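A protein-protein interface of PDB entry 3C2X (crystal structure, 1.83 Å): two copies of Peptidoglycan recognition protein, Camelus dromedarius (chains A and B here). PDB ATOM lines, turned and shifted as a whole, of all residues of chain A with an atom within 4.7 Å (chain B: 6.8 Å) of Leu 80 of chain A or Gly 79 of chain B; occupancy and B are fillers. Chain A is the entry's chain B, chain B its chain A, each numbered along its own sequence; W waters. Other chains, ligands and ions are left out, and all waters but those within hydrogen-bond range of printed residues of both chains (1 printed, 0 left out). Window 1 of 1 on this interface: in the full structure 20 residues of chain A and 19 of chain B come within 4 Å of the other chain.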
ATOM      1  N   VAL A  10      17.466 -12.476   8.696  1.00  0.00           N
ATOM      2  CA  VAL A  10      16.599 -11.321   8.531  1.00  0.00           C
ATOM      3  C   VAL A  10      16.746 -10.541   9.845  1.00  0.00           C
ATOM      4  O   VAL A  10      16.388 -11.036  10.914  1.00  0.00           O
ATOM      5  CB  VAL A  10      15.135 -11.758   8.325  1.00  0.00           C
ATOM      6  CG1 VAL A  10      14.227 -10.544   8.344  1.00  0.00           C
ATOM      7  CG2 VAL A  10      14.986 -12.498   6.992  1.00  0.00           C
ATOM      8  N   PRO A  46       8.475 -14.293   2.540  1.00  0.00           N
ATOM      9  CA  PRO A  46       9.165 -13.324   3.394  1.00  0.00           C
ATOM     10  C   PRO A  46       8.178 -12.369   4.067  1.00  0.00           C
ATOM     11  O   PRO A  46       8.316 -12.049   5.250  1.00  0.00           O
ATOM     12  CB  PRO A  46      10.082 -12.600   2.415  1.00  0.00           C
ATOM     13  CG  PRO A  46      10.418 -13.671   1.421  1.00  0.00           C
ATOM     14  CD  PRO A  46       9.090 -14.360   1.204  1.00  0.00           C
ATOM     15  N   LEU A  74      14.452 -17.611  14.842  1.00  0.00           N
ATOM     16  CA  LEU A  74      13.189 -18.165  14.336  1.00  0.00           C
ATOM     17  C   LEU A  74      13.410 -18.640  12.892  1.00  0.00           C
ATOM     18  O   LEU A  74      14.123 -17.986  12.134  1.00  0.00           O
ATOM     19  CB  LEU A  74      12.080 -17.100  14.330  1.00  0.00           C
ATOM     20  CG  LEU A  74      11.489 -16.427  15.580  1.00  0.00           C
ATOM     21  CD1 LEU A  74      10.423 -17.301  16.188  1.00  0.00           C
ATOM     22  CD2 LEU A  74      12.569 -16.087  16.566  1.00  0.00           C
ATOM     23  N   ILE A  75      12.808 -19.765  12.516  1.00  0.00           N
ATOM     24  CA  ILE A  75      12.945 -20.290  11.156  1.00  0.00           C
ATOM     25  C   ILE A  75      11.587 -20.316  10.460  1.00  0.00           C
ATOM     26  O   ILE A  75      10.606 -20.829  11.007  1.00  0.00           O
ATOM     27  CB  ILE A  75      13.485 -21.741  11.138  1.00  0.00           C
ATOM     28  CG1 ILE A  75      14.597 -21.928  12.175  1.00  0.00           C
ATOM     29  CG2 ILE A  75      14.010 -22.076   9.749  1.00  0.00           C
ATOM     30  CD1 ILE A  75      15.861 -21.145  11.916  1.00  0.00           C
ATOM     31  N   GLY A  76      11.520 -19.779   9.247  1.00  0.00           N
ATOM     32  CA  GLY A  76      10.253 -19.772   8.531  1.00  0.00           C
ATOM     33  C   GLY A  76      10.215 -20.753   7.378  1.00  0.00           C
ATOM     34  O   GLY A  76      11.265 -21.167   6.881  1.00  0.00           O
ATOM     35  N   ASP A  78       9.598 -20.084   4.612  1.00  0.00           N
ATOM     36  CA  ASP A  78      10.035 -19.312   3.449  1.00  0.00           C
ATOM     37  C   ASP A  78      11.518 -19.615   3.266  1.00  0.00           C
ATOM     38  O   ASP A  78      12.156 -19.148   2.328  1.00  0.00           O
ATOM     39  CB  ASP A  78       9.821 -17.804   3.672  1.00  0.00           C
ATOM     40  CG  ASP A  78      10.573 -17.264   4.881  1.00  0.00           C
ATOM     41  OD1 ASP A  78      11.145 -18.058   5.661  1.00  0.00           O
ATOM     42  OD2 ASP A  78      10.585 -16.027   5.060  1.00  0.00           O
ATOM     43  N   GLY A  79      12.065 -20.405   4.181  1.00  0.00           N
ATOM     44  CA  GLY A  79      13.471 -20.765   4.100  1.00  0.00           C
ATOM     45  C   GLY A  79      14.449 -19.718   4.602  1.00  0.00           C
ATOM     46  O   GLY A  79      15.639 -19.781   4.293  1.00  0.00           O
ATOM     47  N   LEU A  80      13.961 -18.756   5.378  1.00  0.00           N
ATOM     48  CA  LEU A  80      14.822 -17.708   5.920  1.00  0.00           C
ATOM     49  C   LEU A  80      14.876 -17.784   7.444  1.00  0.00           C
ATOM     50  O   LEU A  80      13.937 -18.265   8.081  1.00  0.00           O
ATOM     51  CB  LEU A  80      14.298 -16.327   5.517  1.00  0.00           C
ATOM     52  CG  LEU A  80      14.166 -16.022   4.019  1.00  0.00           C
ATOM     53  CD1 LEU A  80      13.618 -14.607   3.843  1.00  0.00           C
ATOM     54  CD2 LEU A  80      15.520 -16.155   3.337  1.00  0.00           C
ATOM     55  N   VAL A  81      15.976 -17.311   8.019  1.00  0.00           N
ATOM     56  CA  VAL A  81      16.131 -17.291   9.464  1.00  0.00           C
ATOM     57  C   VAL A  81      15.836 -15.883   9.932  1.00  0.00           C
ATOM     58  O   VAL A  81      16.242 -14.905   9.281  1.00  0.00           O
ATOM     59  CB  VAL A  81      17.564 -17.641   9.891  1.00  0.00           C
ATOM     60  CG1 VAL A  81      17.694 -17.520  11.405  1.00  0.00           C
ATOM     61  CG2 VAL A  81      17.919 -19.043   9.426  1.00  0.00           C
ATOM     62  N   TYR A  82      15.137 -15.783  11.059  1.00  0.00           N
ATOM     63  CA  TYR A  82      14.785 -14.500  11.639  1.00  0.00           C
ATOM     64  C   TYR A  82      15.527 -14.275  12.947  1.00  0.00           C
ATOM     65  O   TYR A  82      15.526 -15.127  13.830  1.00  0.00           O
ATOM     66  CB  TYR A  82      13.269 -14.418  11.843  1.00  0.00           C
ATOM     67  CG  TYR A  82      12.534 -14.397  10.520  1.00  0.00           C
ATOM     68  CD1 TYR A  82      12.408 -15.557   9.751  1.00  0.00           C
ATOM     69  CD2 TYR A  82      12.079 -13.190   9.978  1.00  0.00           C
ATOM     70  CE1 TYR A  82      11.856 -15.514   8.465  1.00  0.00           C
ATOM     71  CE2 TYR A  82      11.534 -13.133   8.706  1.00  0.00           C
ATOM     72  CZ  TYR A  82      11.427 -14.293   7.951  1.00  0.00           C
ATOM     73  OH  TYR A  82      10.927 -14.235   6.672  1.00  0.00           O
ATOM     74  N   ALA A 123      18.087 -23.694   6.103  1.00  0.00           N
ATOM     75  CA  ALA A 123      18.311 -22.413   6.766  1.00  0.00           C
ATOM     76  C   ALA A 123      18.835 -22.673   8.173  1.00  0.00           C
ATOM     77  O   ALA A 123      19.791 -22.035   8.632  1.00  0.00           O
ATOM     78  CB  ALA A 123      17.002 -21.619   6.827  1.00  0.00           C
ATOM     79  N   CYS B  43      10.553 -12.241  -8.610  1.00  0.00           N
ATOM     80  CA  CYS B  43       9.655 -13.106  -7.842  1.00  0.00           C
ATOM     81  C   CYS B  43      10.017 -12.896  -6.380  1.00  0.00           C
ATOM     82  O   CYS B  43      11.181 -12.654  -6.081  1.00  0.00           O
ATOM     83  CB  CYS B  43       9.923 -14.574  -8.226  1.00  0.00           C
ATOM     84  SG  CYS B  43      11.718 -14.953  -8.179  1.00  0.00           S
ATOM     85  N   ASP B  44       9.050 -12.967  -5.468  1.00  0.00           N
ATOM     86  CA  ASP B  44       9.398 -12.786  -4.064  1.00  0.00           C
ATOM     87  C   ASP B  44       8.938 -13.897  -3.111  1.00  0.00           C
ATOM     88  O   ASP B  44       8.870 -13.700  -1.894  1.00  0.00           O
ATOM     89  CB  ASP B  44       8.950 -11.404  -3.550  1.00  0.00           C
ATOM     90  CG  ASP B  44       7.475 -11.139  -3.746  1.00  0.00           C
ATOM     91  OD1 ASP B  44       6.711 -12.098  -3.958  1.00  0.00           O
ATOM     92  OD2 ASP B  44       7.080  -9.955  -3.668  1.00  0.00           O
ATOM     93  N   THR B  45       8.632 -15.065  -3.665  1.00  0.00           N
ATOM     94  CA  THR B  45       8.255 -16.217  -2.852  1.00  0.00           C
ATOM     95  C   THR B  45       9.018 -17.411  -3.393  1.00  0.00           C
ATOM     96  O   THR B  45       9.375 -17.438  -4.566  1.00  0.00           O
ATOM     97  CB  THR B  45       6.739 -16.538  -2.928  1.00  0.00           C
ATOM     98  OG1 THR B  45       6.428 -17.123  -4.201  1.00  0.00           O
ATOM     99  CG2 THR B  45       5.921 -15.272  -2.720  1.00  0.00           C
ATOM    100  N   CYS B  49       9.874 -18.106  -7.324  1.00  0.00           N
ATOM    101  CA  CYS B  49      11.275 -17.997  -7.694  1.00  0.00           C
ATOM    102  C   CYS B  49      11.826 -19.317  -8.231  1.00  0.00           C
ATOM    103  O   CYS B  49      12.770 -19.332  -9.016  1.00  0.00           O
ATOM    104  CB  CYS B  49      12.089 -17.496  -6.504  1.00  0.00           C
ATOM    105  SG  CYS B  49      12.024 -15.687  -6.297  1.00  0.00           S
ATOM    106  N   ILE B  75      19.917 -15.392  -7.964  1.00  0.00           N
ATOM    107  CA  ILE B  75      19.431 -14.867  -6.696  1.00  0.00           C
ATOM    108  C   ILE B  75      17.996 -14.370  -6.839  1.00  0.00           C
ATOM    109  O   ILE B  75      17.698 -13.572  -7.723  1.00  0.00           O
ATOM    110  CB  ILE B  75      20.285 -13.682  -6.212  1.00  0.00           C
ATOM    111  CG1 ILE B  75      21.785 -13.985  -6.351  1.00  0.00           C
ATOM    112  CG2 ILE B  75      19.905 -13.343  -4.780  1.00  0.00           C
ATOM    113  CD1 ILE B  75      22.328 -15.051  -5.409  1.00  0.00           C
ATOM    114  N   GLY B  76      17.110 -14.835  -5.966  1.00  0.00           N
ATOM    115  CA  GLY B  76      15.728 -14.406  -6.030  1.00  0.00           C
ATOM    116  C   GLY B  76      15.370 -13.350  -5.001  1.00  0.00           C
ATOM    117  O   GLY B  76      16.046 -13.191  -3.978  1.00  0.00           O
ATOM    118  N   GLU B  77      14.304 -12.605  -5.264  1.00  0.00           N
ATOM    119  CA  GLU B  77      13.900 -11.583  -4.315  1.00  0.00           C
ATOM    120  C   GLU B  77      13.216 -12.197  -3.098  1.00  0.00           C
ATOM    121  O   GLU B  77      12.789 -11.485  -2.194  1.00  0.00           O
ATOM    122  CB  GLU B  77      13.024 -10.533  -4.996  1.00  0.00           C
ATOM    123  CG  GLU B  77      13.840  -9.642  -5.937  1.00  0.00           C
ATOM    124  CD  GLU B  77      13.070  -8.442  -6.436  1.00  0.00           C
ATOM    125  OE1 GLU B  77      12.180  -7.959  -5.702  1.00  0.00           O
ATOM    126  OE2 GLU B  77      13.370  -7.973  -7.556  1.00  0.00           O
ATOM    127  N   ASP B  78      13.139 -13.527  -3.085  1.00  0.00           N
ATOM    128  CA  ASP B  78      12.564 -14.267  -1.961  1.00  0.00           C
ATOM    129  C   ASP B  78      13.696 -14.453  -0.954  1.00  0.00           C
ATOM    130  O   ASP B  78      13.510 -14.985   0.144  1.00  0.00           O
ATOM    131  CB  ASP B  78      12.026 -15.628  -2.422  1.00  0.00           C
ATOM    132  CG  ASP B  78      13.085 -16.489  -3.099  1.00  0.00           C
ATOM    133  OD1 ASP B  78      14.194 -15.991  -3.399  1.00  0.00           O
ATOM    134  OD2 ASP B  78      12.796 -17.674  -3.347  1.00  0.00           O
ATOM    135  N   GLY B  79      14.884 -14.005  -1.348  1.00  0.00           N
ATOM    136  CA  GLY B  79      16.039 -14.106  -0.478  1.00  0.00           C
ATOM    137  C   GLY B  79      16.776 -15.428  -0.533  1.00  0.00           C
ATOM    138  O   GLY B  79      17.596 -15.716   0.346  1.00  0.00           O
ATOM    139  N   LEU B  80      16.509 -16.238  -1.553  1.00  0.00           N
ATOM    140  CA  LEU B  80      17.187 -17.521  -1.668  1.00  0.00           C
ATOM    141  C   LEU B  80      18.101 -17.596  -2.890  1.00  0.00           C
ATOM    142  O   LEU B  80      17.874 -16.932  -3.896  1.00  0.00           O
ATOM    143  CB  LEU B  80      16.168 -18.661  -1.738  1.00  0.00           C
ATOM    144  CG  LEU B  80      15.141 -18.773  -0.606  1.00  0.00           C
ATOM    145  CD1 LEU B  80      14.280 -20.005  -0.835  1.00  0.00           C
ATOM    146  CD2 LEU B  80      15.844 -18.874   0.733  1.00  0.00           C
ATOM    147  N   VAL B  81      19.142 -18.411  -2.778  1.00  0.00           N
ATOM    148  CA  VAL B  81      20.087 -18.622  -3.861  1.00  0.00           C
ATOM    149  C   VAL B  81      19.684 -19.904  -4.579  1.00  0.00           C
ATOM    150  O   VAL B  81      19.386 -20.914  -3.935  1.00  0.00           O
ATOM    151  CB  VAL B  81      21.520 -18.782  -3.329  1.00  0.00           C
ATOM    152  CG1 VAL B  81      22.462 -19.114  -4.475  1.00  0.00           C
ATOM    153  CG2 VAL B  81      21.969 -17.501  -2.622  1.00  0.00           C
ATOM    154  N   TYR B  82      19.668 -19.859  -5.906  1.00  0.00           N
ATOM    155  CA  TYR B  82      19.299 -21.013  -6.719  1.00  0.00           C
ATOM    156  C   TYR B  82      20.529 -21.557  -7.451  1.00  0.00           C
ATOM    157  O   TYR B  82      21.212 -20.810  -8.152  1.00  0.00           O
ATOM    158  CB  TYR B  82      18.202 -20.608  -7.718  1.00  0.00           C
ATOM    159  CG  TYR B  82      16.884 -20.293  -7.036  1.00  0.00           C
ATOM    160  CD1 TYR B  82      16.699 -19.085  -6.357  1.00  0.00           C
ATOM    161  CD2 TYR B  82      15.869 -21.253  -6.964  1.00  0.00           C
ATOM    162  CE1 TYR B  82      15.549 -18.845  -5.612  1.00  0.00           C
ATOM    163  CE2 TYR B  82      14.707 -21.021  -6.220  1.00  0.00           C
ATOM    164  CZ  TYR B  82      14.560 -19.815  -5.539  1.00  0.00           C
ATOM    165  OH  TYR B  82      13.459 -19.588  -4.736  1.00  0.00           O
ATOM    166  N   PRO B 117      15.854  -6.510  -2.865  1.00  0.00           N
ATOM    167  CA  PRO B 117      15.647  -6.293  -1.430  1.00  0.00           C
ATOM    168  C   PRO B 117      16.859  -6.712  -0.615  1.00  0.00           C
ATOM    169  O   PRO B 117      17.664  -7.523  -1.067  1.00  0.00           O
ATOM    170  CB  PRO B 117      14.403  -7.130  -1.109  1.00  0.00           C
ATOM    171  CG  PRO B 117      14.281  -8.098  -2.235  1.00  0.00           C
ATOM    172  CD  PRO B 117      14.935  -7.511  -3.433  1.00  0.00           C
ATOM    173  N   ARG B 119      17.295  -8.794   1.647  1.00  0.00           N
ATOM    174  CA  ARG B 119      17.476 -10.243   1.777  1.00  0.00           C
ATOM    175  C   ARG B 119      18.153 -10.861   0.557  1.00  0.00           C
ATOM    176  O   ARG B 119      18.913 -11.824   0.681  1.00  0.00           O
ATOM    177  CB  ARG B 119      16.144 -10.955   2.085  1.00  0.00           C
ATOM    178  CG  ARG B 119      15.096 -10.847   1.015  1.00  0.00           C
ATOM    179  CD  ARG B 119      13.758 -11.498   1.402  1.00  0.00           C
ATOM    180  NE  ARG B 119      12.750 -11.029   0.460  1.00  0.00           N
ATOM    181  CZ  ARG B 119      11.987  -9.965   0.668  1.00  0.00           C
ATOM    182  NH1 ARG B 119      12.095  -9.290   1.798  1.00  0.00           N
ATOM    183  NH2 ARG B 119      11.179  -9.522  -0.290  1.00  0.00           N
ATOM    184  N   ALA B 120      17.907 -10.302  -0.618  1.00  0.00           N
ATOM    185  CA  ALA B 120      18.539 -10.811  -1.825  1.00  0.00           C
ATOM    186  C   ALA B 120      20.024 -10.450  -1.794  1.00  0.00           C
ATOM    187  O   ALA B 120      20.869 -11.277  -2.122  1.00  0.00           O
ATOM    188  CB  ALA B 120      17.873 -10.220  -3.075  1.00  0.00           C
ATOM    189  N   LEU B 121      20.342  -9.222  -1.383  1.00  0.00           N
ATOM    190  CA  LEU B 121      21.730  -8.785  -1.332  1.00  0.00           C
ATOM    191  C   LEU B 121      22.506  -9.630  -0.317  1.00  0.00           C
ATOM    192  O   LEU B 121      23.651 -10.011  -0.564  1.00  0.00           O
ATOM    193  CB  LEU B 121      21.812  -7.294  -0.985  1.00  0.00           C
ATOM    194  CG  LEU B 121      21.084  -6.302  -1.911  1.00  0.00           C
ATOM    195  CD1 LEU B 121      21.281  -4.902  -1.389  1.00  0.00           C
ATOM    196  CD2 LEU B 121      21.604  -6.413  -3.326  1.00  0.00           C
ATOM    197  N   ARG B 122      21.874  -9.946   0.810  1.00  0.00           N
ATOM    198  CA  ARG B 122      22.523 -10.768   1.832  1.00  0.00           C
ATOM    199  C   ARG B 122      22.806 -12.174   1.312  1.00  0.00           C
ATOM    200  O   ARG B 122      23.876 -12.731   1.553  1.00  0.00           O
ATOM    201  CB  ARG B 122      21.644 -10.884   3.091  1.00  0.00           C
ATOM    202  CG  ARG B 122      21.471  -9.600   3.894  1.00  0.00           C
ATOM    203  CD  ARG B 122      20.838  -9.902   5.255  1.00  0.00           C
ATOM    204  NE  ARG B 122      19.445 -10.334   5.168  1.00  0.00           N
ATOM    205  CZ  ARG B 122      18.413  -9.499   5.170  1.00  0.00           C
ATOM    206  NH1 ARG B 122      17.168  -9.966   5.088  1.00  0.00           N
ATOM    207  NH2 ARG B 122      18.624  -8.192   5.272  1.00  0.00           N
ATOM    208  N   ALA B 123      21.839 -12.765   0.615  1.00  0.00           N
ATOM    209  CA  ALA B 123      22.017 -14.113   0.080  1.00  0.00           C
ATOM    210  C   ALA B 123      23.237 -14.154  -0.829  1.00  0.00           C
ATOM    211  O   ALA B 123      24.100 -15.028  -0.701  1.00  0.00           O
ATOM    212  CB  ALA B 123      20.762 -14.548  -0.696  1.00  0.00           C
ATOM    213  N   ALA B 124      23.306 -13.188  -1.739  1.00  0.00           N
ATOM    214  CA  ALA B 124      24.406 -13.082  -2.690  1.00  0.00           C
ATOM    215  C   ALA B 124      25.742 -12.970  -1.969  1.00  0.00           C
ATOM    216  O   ALA B 124      26.671 -13.725  -2.235  1.00  0.00           O
ATOM    217  CB  ALA B 124      24.197 -11.859  -3.589  1.00  0.00           C
HETATM  218  O   HOH W   1      11.712 -16.886   0.873  1.00  0.00           O
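Among the printed residues, merely in contact across the chains: Val 10 of chain A with Arg 122 of chain B (3.7 Å), Pro 46 of chain A with Asp 44 of chain B (3.2 Å), Pro 46 of chain A with Asp 78 of chain B (3.6 Å), Pro 46 of chain A with Arg 119 of chain B (3.7 Å), Asp 78 of chain A with Leu 80 of chain B (3.9 Å), Gly 79 of chain A with Leu 80 of chain B (3.7 Å), Leu 80 of chain A with Asp 78 of chain B (3.7 Å), Leu 80 of chain A with Gly 79 of chain B (3.7 Å), Leu 80 of chain A with Leu 80 of chain B (3.8 Å) and Leu 80 of chain A with Arg 119 of chain B (3.96 Å).
Asp 78 of chain A touches Leu 80 of chain B, and with the chains exchanged Leu 80 of chain A touches Asp 78 of chain B.
Gly 79 of chain A touches Leu 80 of chain B, and with the chains exchanged Leu 80 of chain A touches Gly 79 of chain B.
Leu 80 of chain A touches its own counterpart, Leu 80 of chain B.
Of the 10 pairs that touch across the chains among the printed residues, 5 have their exchanged pair printed and touching as well.
The guanidinium group of Arg 119 of chain B is in hydrogen-bond range of the backbone carbonyl oxygen of Glu 77 of chain B, 2.7 Å away.
N of Leu 80 of chain B sits at hydrogen-bond distance from OD1 of Asp 78 of chain B, at 3.0 Å.
The side-chain carboxylate of Asp 78 of chain B sits at hydrogen-bond distance from the side-chain hydroxyl of Tyr 82 of chain B (2.5 Å).
N of Leu 80 of chain A is in hydrogen-bond range of OD1 of Asp 78 of chain A, at 2.9 Å.
The side-chain hydroxyl (OH) of Tyr 82 of chain A is in hydrogen-bond range of the side-chain carboxylate (OD2) of Asp 78 of chain A (2.4 Å).
The side-chain sulfur (SG) of Cys 49 of chain B forms a disulfide with the side-chain sulfur (SG) of Cys 43 of chain B, 2.0 Å away.
Of the 11 printed residues of chain A, 5 touch a printed residue of chain B.
Printed residues of chain A that touch a printed residue of chain B: Val 10, Pro 46, Asp 78, Gly 79 and Leu 80.
Hydrophobic or aromatic side chains of chain A that line the printed part of chain B: Val 10, Pro 46 and Leu 80.
Among the printed residues, no Asp or Glu carboxylate lies within 4 Å of a Lys or Arg side-chain nitrogen of the other chain.
Water W1 lies within hydrogen-bond range of the backbone carbonyl oxygen of Asp 78 of chain B and the backbone carbonyl oxygen of Asp 78 of chain A.
Of chain B, only Asp 78 (3.7 Å), Gly 79 (3.7 Å), Leu 80 (3.8 Å) and Arg 119 (3.96 Å) come within 4 Å of Leu 80 of chain A.
Gly 79 of chain B touches just one residue of chain A: Leu 80.
Printed residues of chain A within 4 Å of Asp 44 of chain B: Pro 46.
Of the printed residues of chain B, Gly 79 of chain A touches Leu 80 (3.7 Å).
Printed residues of chain A within 4 Å of Arg 122 of chain B: Val 10 (3.7 Å).
Of the printed residues of chain A, Arg 119 of chain B touches Pro 46 (3.7 Å) and Leu 80 (3.96 Å).
Printed residues of chain B within 4 Å of Asp 78 of chain A: Leu 80 (3.9 Å).
The nearest printed residue of chain A that does not touch Asp 78 of chain B is Asp 78 of chain A (4.9 Å).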
